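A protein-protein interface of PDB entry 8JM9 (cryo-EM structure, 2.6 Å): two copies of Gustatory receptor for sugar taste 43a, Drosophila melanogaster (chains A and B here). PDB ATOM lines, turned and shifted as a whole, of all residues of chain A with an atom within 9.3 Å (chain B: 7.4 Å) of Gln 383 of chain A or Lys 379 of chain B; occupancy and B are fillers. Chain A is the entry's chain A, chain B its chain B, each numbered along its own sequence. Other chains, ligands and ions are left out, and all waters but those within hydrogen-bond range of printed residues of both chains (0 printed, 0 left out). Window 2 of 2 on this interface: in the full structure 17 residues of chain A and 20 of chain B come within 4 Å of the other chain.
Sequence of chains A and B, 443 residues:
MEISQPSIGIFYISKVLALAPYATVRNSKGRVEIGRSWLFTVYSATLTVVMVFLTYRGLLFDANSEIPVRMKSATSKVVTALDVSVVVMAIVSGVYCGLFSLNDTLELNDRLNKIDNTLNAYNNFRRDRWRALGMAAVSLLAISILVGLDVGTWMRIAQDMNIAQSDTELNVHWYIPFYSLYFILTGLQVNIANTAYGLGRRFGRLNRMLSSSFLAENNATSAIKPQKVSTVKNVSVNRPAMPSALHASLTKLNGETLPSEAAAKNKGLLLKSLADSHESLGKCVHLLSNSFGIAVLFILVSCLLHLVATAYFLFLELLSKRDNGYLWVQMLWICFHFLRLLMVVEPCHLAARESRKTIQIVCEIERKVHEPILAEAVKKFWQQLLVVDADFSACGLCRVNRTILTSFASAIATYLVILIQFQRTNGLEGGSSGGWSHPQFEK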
ATOM      1  N   ALA A 275       6.489   2.547 -12.747  1.00  0.00           N
ATOM      2  CA  ALA A 275       6.989   1.181 -12.861  1.00  0.00           C
ATOM      3  C   ALA A 275       7.182   0.553 -11.488  1.00  0.00           C
ATOM      4  O   ALA A 275       6.838  -0.617 -11.271  1.00  0.00           O
ATOM      5  CB  ALA A 275       8.300   1.168 -13.644  1.00  0.00           C
ATOM      6  N   ILE A 359       1.526  -3.875 -20.055  1.00  0.00           N
ATOM      7  CA  ILE A 359       2.597  -4.145 -21.009  1.00  0.00           C
ATOM      8  C   ILE A 359       2.236  -3.597 -22.381  1.00  0.00           C
ATOM      9  O   ILE A 359       3.091  -3.057 -23.090  1.00  0.00           O
ATOM     10  CB  ILE A 359       2.914  -5.649 -21.064  1.00  0.00           C
ATOM     11  CG1 ILE A 359       4.279  -5.866 -21.720  1.00  0.00           C
ATOM     12  CG2 ILE A 359       1.842  -6.398 -21.830  1.00  0.00           C
ATOM     13  CD1 ILE A 359       4.802  -7.274 -21.589  1.00  0.00           C
ATOM     14  N   VAL A 362       2.713   0.108 -22.246  1.00  0.00           N
ATOM     15  CA  VAL A 362       4.130   0.454 -22.265  1.00  0.00           C
ATOM     16  C   VAL A 362       4.717   0.248 -23.654  1.00  0.00           C
ATOM     17  O   VAL A 362       5.600   0.998 -24.080  1.00  0.00           O
ATOM     18  CB  VAL A 362       4.890  -0.358 -21.203  1.00  0.00           C
ATOM     19  CG1 VAL A 362       6.384  -0.306 -21.462  1.00  0.00           C
ATOM     20  CG2 VAL A 362       4.572   0.170 -19.820  1.00  0.00           C
ATOM     21  N   CYS A 363       4.267  -0.780 -24.373  1.00  0.00           N
ATOM     22  CA  CYS A 363       4.722  -0.961 -25.748  1.00  0.00           C
ATOM     23  C   CYS A 363       4.325   0.229 -26.609  1.00  0.00           C
ATOM     24  O   CYS A 363       5.128   0.723 -27.412  1.00  0.00           O
ATOM     25  CB  CYS A 363       4.150  -2.252 -26.332  1.00  0.00           C
ATOM     26  SG  CYS A 363       4.902  -3.761 -25.696  1.00  0.00           S
ATOM     27  N   GLU A 366       6.601   3.093 -25.725  1.00  0.00           N
ATOM     28  CA  GLU A 366       7.925   2.896 -26.302  1.00  0.00           C
ATOM     29  C   GLU A 366       7.929   3.241 -27.783  1.00  0.00           C
ATOM     30  O   GLU A 366       8.843   3.914 -28.271  1.00  0.00           O
ATOM     31  CB  GLU A 366       8.371   1.450 -26.093  1.00  0.00           C
ATOM     32  CG  GLU A 366       9.592   1.049 -26.895  1.00  0.00           C
ATOM     33  CD  GLU A 366      10.263  -0.192 -26.342  1.00  0.00           C
ATOM     34  OE1 GLU A 366       9.547  -1.172 -26.047  1.00  0.00           O
ATOM     35  OE2 GLU A 366      11.504  -0.190 -26.203  1.00  0.00           O
ATOM     36  N   ALA A 375      13.371   6.876 -23.169  1.00  0.00           N
ATOM     37  CA  ALA A 375      13.367   5.622 -23.914  1.00  0.00           C
ATOM     38  C   ALA A 375      13.997   4.501 -23.100  1.00  0.00           C
ATOM     39  O   ALA A 375      13.488   3.375 -23.081  1.00  0.00           O
ATOM     40  CB  ALA A 375      14.099   5.795 -25.244  1.00  0.00           C
ATOM     41  N   GLU A 376      15.110   4.787 -22.422  1.00  0.00           N
ATOM     42  CA  GLU A 376      15.738   3.769 -21.587  1.00  0.00           C
ATOM     43  C   GLU A 376      14.835   3.369 -20.429  1.00  0.00           C
ATOM     44  O   GLU A 376      14.736   2.180 -20.102  1.00  0.00           O
ATOM     45  CB  GLU A 376      17.088   4.280 -21.075  1.00  0.00           C
ATOM     46  CG  GLU A 376      17.658   3.536 -19.869  1.00  0.00           C
ATOM     47  CD  GLU A 376      18.093   2.121 -20.204  1.00  0.00           C
ATOM     48  OE1 GLU A 376      19.087   1.649 -19.612  1.00  0.00           O
ATOM     49  OE2 GLU A 376      17.446   1.481 -21.058  1.00  0.00           O
ATOM     50  N   ALA A 377      14.172   4.339 -19.797  1.00  0.00           N
ATOM     51  CA  ALA A 377      13.260   4.012 -18.707  1.00  0.00           C
ATOM     52  C   ALA A 377      12.109   3.145 -19.199  1.00  0.00           C
ATOM     53  O   ALA A 377      11.707   2.190 -18.525  1.00  0.00           O
ATOM     54  CB  ALA A 377      12.729   5.293 -18.065  1.00  0.00           C
ATOM     55  N   VAL A 378      11.569   3.460 -20.376  1.00  0.00           N
ATOM     56  CA  VAL A 378      10.469   2.674 -20.919  1.00  0.00           C
ATOM     57  C   VAL A 378      10.943   1.272 -21.279  1.00  0.00           C
ATOM     58  O   VAL A 378      10.205   0.297 -21.117  1.00  0.00           O
ATOM     59  CB  VAL A 378       9.850   3.393 -22.130  1.00  0.00           C
ATOM     60  CG1 VAL A 378       8.778   2.531 -22.761  1.00  0.00           C
ATOM     61  CG2 VAL A 378       9.261   4.728 -21.710  1.00  0.00           C
ATOM     62  N   LYS A 379      12.170   1.147 -21.787  1.00  0.00           N
ATOM     63  CA  LYS A 379      12.713  -0.178 -22.073  1.00  0.00           C
ATOM     64  C   LYS A 379      12.838  -0.983 -20.786  1.00  0.00           C
ATOM     65  O   LYS A 379      12.460  -2.161 -20.738  1.00  0.00           O
ATOM     66  CB  LYS A 379      14.066  -0.028 -22.778  1.00  0.00           C
ATOM     67  CG  LYS A 379      15.077  -1.196 -22.714  1.00  0.00           C
ATOM     68  CD  LYS A 379      14.487  -2.603 -22.862  1.00  0.00           C
ATOM     69  CE  LYS A 379      13.651  -2.748 -24.122  1.00  0.00           C
ATOM     70  NZ  LYS A 379      14.396  -2.335 -25.340  1.00  0.00           N
ATOM     71  N   LYS A 380      13.337  -0.355 -19.719  1.00  0.00           N
ATOM     72  CA  LYS A 380      13.438  -1.048 -18.440  1.00  0.00           C
ATOM     73  C   LYS A 380      12.064  -1.486 -17.947  1.00  0.00           C
ATOM     74  O   LYS A 380      11.897  -2.611 -17.460  1.00  0.00           O
ATOM     75  CB  LYS A 380      14.111  -0.144 -17.408  1.00  0.00           C
ATOM     76  CG  LYS A 380      15.547   0.226 -17.742  1.00  0.00           C
ATOM     77  CD  LYS A 380      16.544  -0.639 -16.988  1.00  0.00           C
ATOM     78  CE  LYS A 380      16.526  -2.075 -17.485  1.00  0.00           C
ATOM     79  NZ  LYS A 380      17.630  -2.883 -16.901  1.00  0.00           N
ATOM     80  N   PHE A 381      11.069  -0.606 -18.066  1.00  0.00           N
ATOM     81  CA  PHE A 381       9.718  -0.947 -17.636  1.00  0.00           C
ATOM     82  C   PHE A 381       9.157  -2.106 -18.452  1.00  0.00           C
ATOM     83  O   PHE A 381       8.514  -3.008 -17.906  1.00  0.00           O
ATOM     84  CB  PHE A 381       8.821   0.286 -17.752  1.00  0.00           C
ATOM     85  CG  PHE A 381       7.495   0.162 -17.048  1.00  0.00           C
ATOM     86  CD1 PHE A 381       7.198  -0.929 -16.248  1.00  0.00           C
ATOM     87  CD2 PHE A 381       6.546   1.156 -17.183  1.00  0.00           C
ATOM     88  CE1 PHE A 381       5.982  -1.024 -15.610  1.00  0.00           C
ATOM     89  CE2 PHE A 381       5.330   1.064 -16.545  1.00  0.00           C
ATOM     90  CZ  PHE A 381       5.048  -0.026 -15.758  1.00  0.00           C
ATOM     91  N   TRP A 382       9.386  -2.094 -19.766  1.00  0.00           N
ATOM     92  CA  TRP A 382       8.914  -3.184 -20.612  1.00  0.00           C
ATOM     93  C   TRP A 382       9.570  -4.500 -20.222  1.00  0.00           C
ATOM     94  O   TRP A 382       8.906  -5.541 -20.156  1.00  0.00           O
ATOM     95  CB  TRP A 382       9.197  -2.859 -22.078  1.00  0.00           C
ATOM     96  CG  TRP A 382       8.771  -3.931 -23.026  1.00  0.00           C
ATOM     97  CD1 TRP A 382       7.550  -4.067 -23.612  1.00  0.00           C
ATOM     98  CD2 TRP A 382       9.568  -5.022 -23.500  1.00  0.00           C
ATOM     99  NE1 TRP A 382       7.534  -5.175 -24.422  1.00  0.00           N
ATOM    100  CE2 TRP A 382       8.761  -5.779 -24.370  1.00  0.00           C
ATOM    101  CE3 TRP A 382      10.885  -5.432 -23.273  1.00  0.00           C
ATOM    102  CZ2 TRP A 382       9.228  -6.921 -25.014  1.00  0.00           C
ATOM    103  CZ3 TRP A 382      11.344  -6.567 -23.912  1.00  0.00           C
ATOM    104  CH2 TRP A 382      10.519  -7.298 -24.772  1.00  0.00           C
ATOM    105  N   GLN A 383      10.878  -4.475 -19.963  1.00  0.00           N
ATOM    106  CA  GLN A 383      11.563  -5.692 -19.543  1.00  0.00           C
ATOM    107  C   GLN A 383      11.011  -6.195 -18.218  1.00  0.00           C
ATOM    108  O   GLN A 383      10.831  -7.403 -18.029  1.00  0.00           O
ATOM    109  CB  GLN A 383      13.066  -5.441 -19.437  1.00  0.00           C
ATOM    110  CG  GLN A 383      13.891  -6.247 -20.422  1.00  0.00           C
ATOM    111  CD  GLN A 383      15.378  -6.036 -20.239  1.00  0.00           C
ATOM    112  OE1 GLN A 383      15.805  -5.151 -19.498  1.00  0.00           O
ATOM    113  NE2 GLN A 383      16.179  -6.852 -20.915  1.00  0.00           N
ATOM    114  N   GLN A 384      10.737  -5.281 -17.286  1.00  0.00           N
ATOM    115  CA  GLN A 384      10.145  -5.678 -16.015  1.00  0.00           C
ATOM    116  C   GLN A 384       8.784  -6.327 -16.227  1.00  0.00           C
ATOM    117  O   GLN A 384       8.486  -7.370 -15.635  1.00  0.00           O
ATOM    118  CB  GLN A 384      10.031  -4.459 -15.099  1.00  0.00           C
ATOM    119  CG  GLN A 384       9.050  -4.597 -13.947  1.00  0.00           C
ATOM    120  CD  GLN A 384       8.881  -3.304 -13.183  1.00  0.00           C
ATOM    121  OE1 GLN A 384       9.847  -2.580 -12.945  1.00  0.00           O
ATOM    122  NE2 GLN A 384       7.648  -3.000 -12.800  1.00  0.00           N
ATOM    123  N   LEU A 385       7.948  -5.729 -17.077  1.00  0.00           N
ATOM    124  CA  LEU A 385       6.611  -6.258 -17.313  1.00  0.00           C
ATOM    125  C   LEU A 385       6.633  -7.571 -18.077  1.00  0.00           C
ATOM    126  O   LEU A 385       5.673  -8.342 -17.989  1.00  0.00           O
ATOM    127  CB  LEU A 385       5.773  -5.242 -18.087  1.00  0.00           C
ATOM    128  CG  LEU A 385       5.417  -3.961 -17.339  1.00  0.00           C
ATOM    129  CD1 LEU A 385       4.785  -2.967 -18.285  1.00  0.00           C
ATOM    130  CD2 LEU A 385       4.488  -4.258 -16.182  1.00  0.00           C
ATOM    131  N   LEU A 386       7.696  -7.838 -18.833  1.00  0.00           N
ATOM    132  CA  LEU A 386       7.744  -9.060 -19.625  1.00  0.00           C
ATOM    133  C   LEU A 386       7.652 -10.313 -18.764  1.00  0.00           C
ATOM    134  O   LEU A 386       7.191 -11.350 -19.252  1.00  0.00           O
ATOM    135  CB  LEU A 386       9.033  -9.076 -20.455  1.00  0.00           C
ATOM    136  CG  LEU A 386       9.138  -9.969 -21.699  1.00  0.00           C
ATOM    137  CD1 LEU A 386       9.490 -11.406 -21.335  1.00  0.00           C
ATOM    138  CD2 LEU A 386       7.859  -9.928 -22.526  1.00  0.00           C
ATOM    139  N   VAL A 387       8.046 -10.241 -17.493  1.00  0.00           N
ATOM    140  CA  VAL A 387       8.185 -11.437 -16.667  1.00  0.00           C
ATOM    141  C   VAL A 387       7.378 -11.340 -15.377  1.00  0.00           C
ATOM    142  O   VAL A 387       7.674 -12.039 -14.402  1.00  0.00           O
ATOM    143  CB  VAL A 387       9.669 -11.701 -16.351  1.00  0.00           C
ATOM    144  CG1 VAL A 387      10.517 -11.501 -17.590  1.00  0.00           C
ATOM    145  CG2 VAL A 387      10.154 -10.789 -15.231  1.00  0.00           C
ATOM    146  N   VAL A 388       6.350 -10.501 -15.357  1.00  0.00           N
ATOM    147  CA  VAL A 388       5.528 -10.371 -14.158  1.00  0.00           C
ATOM    148  C   VAL A 388       4.525 -11.513 -14.101  1.00  0.00           C
ATOM    149  O   VAL A 388       3.980 -11.949 -15.120  1.00  0.00           O
ATOM    150  CB  VAL A 388       4.809  -9.006 -14.108  1.00  0.00           C
ATOM    151  CG1 VAL A 388       5.790  -7.903 -13.761  1.00  0.00           C
ATOM    152  CG2 VAL A 388       4.097  -8.714 -15.417  1.00  0.00           C
ATOM    153  N   LEU B 271      28.506 -13.526  -8.772  1.00  0.00           N
ATOM    154  CA  LEU B 271      27.244 -13.622  -9.496  1.00  0.00           C
ATOM    155  C   LEU B 271      27.305 -14.682 -10.586  1.00  0.00           C
ATOM    156  O   LEU B 271      26.321 -15.393 -10.812  1.00  0.00           O
ATOM    157  CB  LEU B 271      26.868 -12.275 -10.108  1.00  0.00           C
ATOM    158  CG  LEU B 271      25.450 -12.253 -10.677  1.00  0.00           C
ATOM    159  CD1 LEU B 271      24.728 -10.985 -10.270  1.00  0.00           C
ATOM    160  CD2 LEU B 271      25.477 -12.392 -12.187  1.00  0.00           C
ATOM    161  N   VAL B 362      16.669 -11.397  -9.759  1.00  0.00           N
ATOM    162  CA  VAL B 362      17.665 -10.904 -10.703  1.00  0.00           C
ATOM    163  C   VAL B 362      17.187  -9.624 -11.373  1.00  0.00           C
ATOM    164  O   VAL B 362      17.988  -8.734 -11.671  1.00  0.00           O
ATOM    165  CB  VAL B 362      18.003 -11.992 -11.736  1.00  0.00           C
ATOM    166  CG1 VAL B 362      18.723 -11.389 -12.927  1.00  0.00           C
ATOM    167  CG2 VAL B 362      18.850 -13.071 -11.095  1.00  0.00           C
ATOM    168  N   CYS B 363      15.888  -9.515 -11.650  1.00  0.00           N
ATOM    169  CA  CYS B 363      15.362  -8.269 -12.198  1.00  0.00           C
ATOM    170  C   CYS B 363      15.578  -7.118 -11.226  1.00  0.00           C
ATOM    171  O   CYS B 363      15.981  -6.019 -11.629  1.00  0.00           O
ATOM    172  CB  CYS B 363      13.877  -8.415 -12.523  1.00  0.00           C
ATOM    173  SG  CYS B 363      13.523  -9.414 -13.981  1.00  0.00           S
ATOM    174  N   GLU B 366      19.225  -6.192 -11.342  1.00  0.00           N
ATOM    175  CA  GLU B 366      19.529  -5.450 -12.558  1.00  0.00           C
ATOM    176  C   GLU B 366      19.079  -4.003 -12.439  1.00  0.00           C
ATOM    177  O   GLU B 366      19.815  -3.081 -12.810  1.00  0.00           O
ATOM    178  CB  GLU B 366      18.854  -6.119 -13.754  1.00  0.00           C
ATOM    179  CG  GLU B 366      18.856  -5.286 -15.020  1.00  0.00           C
ATOM    180  CD  GLU B 366      18.607  -6.120 -16.260  1.00  0.00           C
ATOM    181  OE1 GLU B 366      17.673  -6.949 -16.240  1.00  0.00           O
ATOM    182  OE2 GLU B 366      19.342  -5.949 -17.255  1.00  0.00           O
ATOM    183  N   ILE B 373      30.688  -4.393 -15.743  1.00  0.00           N
ATOM    184  CA  ILE B 373      30.881  -5.840 -15.713  1.00  0.00           C
ATOM    185  C   ILE B 373      29.739  -6.512 -14.961  1.00  0.00           C
ATOM    186  O   ILE B 373      29.185  -7.524 -15.410  1.00  0.00           O
ATOM    187  CB  ILE B 373      32.249  -6.193 -15.101  1.00  0.00           C
ATOM    188  CG1 ILE B 373      32.453  -5.494 -13.750  1.00  0.00           C
ATOM    189  CG2 ILE B 373      33.368  -5.813 -16.059  1.00  0.00           C
ATOM    190  CD1 ILE B 373      33.725  -5.901 -13.041  1.00  0.00           C
ATOM    191  N   LEU B 374      29.365  -5.958 -13.807  1.00  0.00           N
ATOM    192  CA  LEU B 374      28.271  -6.535 -13.036  1.00  0.00           C
ATOM    193  C   LEU B 374      26.954  -6.429 -13.790  1.00  0.00           C
ATOM    194  O   LEU B 374      26.143  -7.360 -13.764  1.00  0.00           O
ATOM    195  CB  LEU B 374      28.169  -5.850 -11.675  1.00  0.00           C
ATOM    196  CG  LEU B 374      27.639  -6.722 -10.536  1.00  0.00           C
ATOM    197  CD1 LEU B 374      28.664  -7.769 -10.137  1.00  0.00           C
ATOM    198  CD2 LEU B 374      27.260  -5.865  -9.341  1.00  0.00           C
ATOM    199  N   ALA B 375      26.717  -5.302 -14.463  1.00  0.00           N
ATOM    200  CA  ALA B 375      25.488  -5.157 -15.233  1.00  0.00           C
ATOM    201  C   ALA B 375      25.423  -6.183 -16.356  1.00  0.00           C
ATOM    202  O   ALA B 375      24.369  -6.779 -16.603  1.00  0.00           O
ATOM    203  CB  ALA B 375      25.381  -3.740 -15.795  1.00  0.00           C
ATOM    204  N   GLU B 376      26.541  -6.401 -17.052  1.00  0.00           N
ATOM    205  CA  GLU B 376      26.557  -7.403 -18.112  1.00  0.00           C
ATOM    206  C   GLU B 376      26.333  -8.802 -17.553  1.00  0.00           C
ATOM    207  O   GLU B 376      25.599  -9.598 -18.152  1.00  0.00           O
ATOM    208  CB  GLU B 376      27.882  -7.327 -18.876  1.00  0.00           C
ATOM    209  CG  GLU B 376      28.232  -8.560 -19.708  1.00  0.00           C
ATOM    210  CD  GLU B 376      27.318  -8.738 -20.907  1.00  0.00           C
ATOM    211  OE1 GLU B 376      27.800  -9.217 -21.955  1.00  0.00           O
ATOM    212  OE2 GLU B 376      26.121  -8.399 -20.805  1.00  0.00           O
ATOM    213  N   ALA B 377      26.951  -9.121 -16.415  1.00  0.00           N
ATOM    214  CA  ALA B 377      26.741 -10.431 -15.810  1.00  0.00           C
ATOM    215  C   ALA B 377      25.284 -10.623 -15.414  1.00  0.00           C
ATOM    216  O   ALA B 377      24.714 -11.702 -15.612  1.00  0.00           O
ATOM    217  CB  ALA B 377      27.653 -10.600 -14.596  1.00  0.00           C
ATOM    218  N   VAL B 378      24.662  -9.584 -14.856  1.00  0.00           N
ATOM    219  CA  VAL B 378      23.265  -9.686 -14.456  1.00  0.00           C
ATOM    220  C   VAL B 378      22.369  -9.827 -15.680  1.00  0.00           C
ATOM    221  O   VAL B 378      21.365 -10.543 -15.646  1.00  0.00           O
ATOM    222  CB  VAL B 378      22.868  -8.472 -13.599  1.00  0.00           C
ATOM    223  CG1 VAL B 378      21.392  -8.520 -13.271  1.00  0.00           C
ATOM    224  CG2 VAL B 378      23.682  -8.437 -12.318  1.00  0.00           C
ATOM    225  N   LYS B 379      22.704  -9.141 -16.773  1.00  0.00           N
ATOM    226  CA  LYS B 379      21.935  -9.300 -18.003  1.00  0.00           C
ATOM    227  C   LYS B 379      22.041 -10.734 -18.507  1.00  0.00           C
ATOM    228  O   LYS B 379      21.036 -11.346 -18.889  1.00  0.00           O
ATOM    229  CB  LYS B 379      22.438  -8.297 -19.047  1.00  0.00           C
ATOM    230  CG  LYS B 379      22.195  -8.590 -20.546  1.00  0.00           C
ATOM    231  CD  LYS B 379      20.823  -9.173 -20.901  1.00  0.00           C
ATOM    232  CE  LYS B 379      19.681  -8.318 -20.377  1.00  0.00           C
ATOM    233  NZ  LYS B 379      19.801  -6.899 -20.803  1.00  0.00           N
ATOM    234  N   LYS B 380      23.249 -11.300 -18.485  1.00  0.00           N
ATOM    235  CA  LYS B 380      23.417 -12.687 -18.904  1.00  0.00           C
ATOM    236  C   LYS B 380      22.602 -13.626 -18.023  1.00  0.00           C
ATOM    237  O   LYS B 380      21.951 -14.553 -18.521  1.00  0.00           O
ATOM    238  CB  LYS B 380      24.896 -13.069 -18.863  1.00  0.00           C
ATOM    239  CG  LYS B 380      25.772 -12.284 -19.826  1.00  0.00           C
ATOM    240  CD  LYS B 380      26.057 -13.066 -21.098  1.00  0.00           C
ATOM    241  CE  LYS B 380      24.808 -13.217 -21.952  1.00  0.00           C
ATOM    242  NZ  LYS B 380      25.111 -13.801 -23.286  1.00  0.00           N
ATOM    243  N   PHE B 381      22.626 -13.397 -16.710  1.00  0.00           N
ATOM    244  CA  PHE B 381      21.861 -14.235 -15.793  1.00  0.00           C
ATOM    245  C   PHE B 381      20.365 -14.120 -16.062  1.00  0.00           C
ATOM    246  O   PHE B 381      19.643 -15.123 -16.041  1.00  0.00           O
ATOM    247  CB  PHE B 381      22.188 -13.843 -14.352  1.00  0.00           C
ATOM    248  CG  PHE B 381      21.716 -14.828 -13.314  1.00  0.00           C
ATOM    249  CD1 PHE B 381      21.167 -16.048 -13.670  1.00  0.00           C
ATOM    250  CD2 PHE B 381      21.838 -14.528 -11.971  1.00  0.00           C
ATOM    251  CE1 PHE B 381      20.744 -16.938 -12.708  1.00  0.00           C
ATOM    252  CE2 PHE B 381      21.418 -15.416 -11.008  1.00  0.00           C
ATOM    253  CZ  PHE B 381      20.870 -16.621 -11.376  1.00  0.00           C
ATOM    254  N   TRP B 382      19.881 -12.903 -16.311  1.00  0.00           N
ATOM    255  CA  TRP B 382      18.468 -12.713 -16.614  1.00  0.00           C
ATOM    256  C   TRP B 382      18.082 -13.438 -17.894  1.00  0.00           C
ATOM    257  O   TRP B 382      17.027 -14.078 -17.964  1.00  0.00           O
ATOM    258  CB  TRP B 382      18.161 -11.220 -16.731  1.00  0.00           C
ATOM    259  CG  TRP B 382      16.737 -10.922 -17.066  1.00  0.00           C
ATOM    260  CD1 TRP B 382      15.710 -10.750 -16.189  1.00  0.00           C
ATOM    261  CD2 TRP B 382      16.180 -10.760 -18.375  1.00  0.00           C
ATOM    262  NE1 TRP B 382      14.546 -10.491 -16.869  1.00  0.00           N
ATOM    263  CE2 TRP B 382      14.808 -10.492 -18.212  1.00  0.00           C
ATOM    264  CE3 TRP B 382      16.708 -10.816 -19.667  1.00  0.00           C
ATOM    265  CZ2 TRP B 382      13.957 -10.280 -19.294  1.00  0.00           C
ATOM    266  CZ3 TRP B 382      15.861 -10.606 -20.738  1.00  0.00           C
ATOM    267  CH2 TRP B 382      14.502 -10.341 -20.545  1.00  0.00           C
ATOM    268  N   GLN B 383      18.924 -13.347 -18.923  1.00  0.00           N
ATOM    269  CA  GLN B 383      18.638 -14.051 -20.168  1.00  0.00           C
ATOM    270  C   GLN B 383      18.609 -15.556 -19.945  1.00  0.00           C
ATOM    271  O   GLN B 383      17.755 -16.257 -20.496  1.00  0.00           O
ATOM    272  CB  GLN B 383      19.673 -13.687 -21.230  1.00  0.00           C
ATOM    273  CG  GLN B 383      19.092 -12.951 -22.422  1.00  0.00           C
ATOM    274  CD  GLN B 383      20.125 -12.674 -23.492  1.00  0.00           C
ATOM    275  OE1 GLN B 383      21.323 -12.866 -23.278  1.00  0.00           O
ATOM    276  NE2 GLN B 383      19.669 -12.221 -24.653  1.00  0.00           N
ATOM    277  N   GLN B 384      19.538 -16.069 -19.138  1.00  0.00           N
ATOM    278  CA  GLN B 384      19.537 -17.493 -18.822  1.00  0.00           C
ATOM    279  C   GLN B 384      18.250 -17.892 -18.114  1.00  0.00           C
ATOM    280  O   GLN B 384      17.636 -18.910 -18.452  1.00  0.00           O
ATOM    281  CB  GLN B 384      20.758 -17.830 -17.967  1.00  0.00           C
ATOM    282  CG  GLN B 384      20.672 -19.135 -17.193  1.00  0.00           C
ATOM    283  CD  GLN B 384      21.845 -19.322 -16.257  1.00  0.00           C
ATOM    284  OE1 GLN B 384      22.984 -19.008 -16.601  1.00  0.00           O
ATOM    285  NE2 GLN B 384      21.573 -19.827 -15.062  1.00  0.00           N
ATOM    286  N   LEU B 385      17.820 -17.097 -17.133  1.00  0.00           N
ATOM    287  CA  LEU B 385      16.619 -17.420 -16.374  1.00  0.00           C
ATOM    288  C   LEU B 385      15.353 -17.276 -17.202  1.00  0.00           C
ATOM    289  O   LEU B 385      14.337 -17.895 -16.874  1.00  0.00           O
ATOM    290  CB  LEU B 385      16.517 -16.522 -15.143  1.00  0.00           C
ATOM    291  CG  LEU B 385      17.573 -16.744 -14.065  1.00  0.00           C
ATOM    292  CD1 LEU B 385      17.485 -15.653 -13.023  1.00  0.00           C
ATOM    293  CD2 LEU B 385      17.406 -18.105 -13.425  1.00  0.00           C
ATOM    294  N   LEU B 386      15.384 -16.467 -18.259  1.00  0.00           N
ATOM    295  CA  LEU B 386      14.184 -16.255 -19.057  1.00  0.00           C
ATOM    296  C   LEU B 386      13.659 -17.548 -19.670  1.00  0.00           C
ATOM    297  O   LEU B 386      12.456 -17.649 -19.931  1.00  0.00           O
ATOM    298  CB  LEU B 386      14.478 -15.225 -20.153  1.00  0.00           C
ATOM    299  CG  LEU B 386      13.326 -14.467 -20.828  1.00  0.00           C
ATOM    300  CD1 LEU B 386      12.680 -15.290 -21.935  1.00  0.00           C
ATOM    301  CD2 LEU B 386      12.280 -14.024 -19.814  1.00  0.00           C
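The side-chain amino group (NZ) of Lys 380 of chain A is in salt-bridge range of the side-chain carboxylate (OE2) of Glu 366 of chain B, 3.5 Å away.
The indole nitrogen (NE1) of Trp 382 of chain B sits at hydrogen-bond distance from the side-chain sulfur (SG) of Cys 363 of chain B (3.2 Å). The side-chain carboxylate (OE2) of Glu 366 of chain B lies within salt-bridge range of the side-chain amino group (NZ) of Lys 379 of chain B, 3.7 Å away.
Among the printed residues, merely in contact across the chains: Gln 383 of chain A with Lys 379 of chain B (3.6 Å), Gln 383 of chain A with Trp 382 of chain B (3.8 Å), Val 387 of chain A with Leu 386 of chain B (3.8 Å) and Val 387 of chain A with Cys 363 of chain B (3.8 Å).
Gln 383 of chain A touches two residues of chain B. Lys 379 of chain B touches just one residue of chain A: Gln 383 (3.6 Å). No residue of chain A comes within 4 Å of Val 378 of chain B. Printed residues of chain A within 4 Å of Cys 363 of chain B: Val 387 (3.8 Å). Of the printed residues of chain B, Val 387 of chain A touches Cys 363 (3.8 Å) and Leu 386 (3.8 Å).
Of the 19 printed residues of chain A, 3 touch a printed residue of chain B. Among the printed residues, Asp or Glu carboxylates within 4 Å of a Lys or Arg side-chain nitrogen of the other chain: Lys 380 of chain A with Glu 366 of chain B (3.5 Å).
Lys 380 of chain A touches Glu 366 of chain B, but with the chains exchanged Glu 366 of chain A does not touch Lys 380 of chain B (17.9 Å). Gln 383 of chain A touches Lys 379 of chain B, but with the chains exchanged Lys 379 of chain A does not touch Gln 383 of chain B (11.1 Å). Gln 383 of chain A touches Trp 382 of chain B, but with the chains exchanged Trp 382 of chain A does not touch Gln 383 of chain B (10.1 Å). Positions printed for both chains: 362, 363, 366, 375, 376, 377, 378, 379, 380, 381, 382, 383, 384, 385 and 386. Of the 5 pairs that touch across the chains among the printed residues, none has its exchanged pair printed and touching as well.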
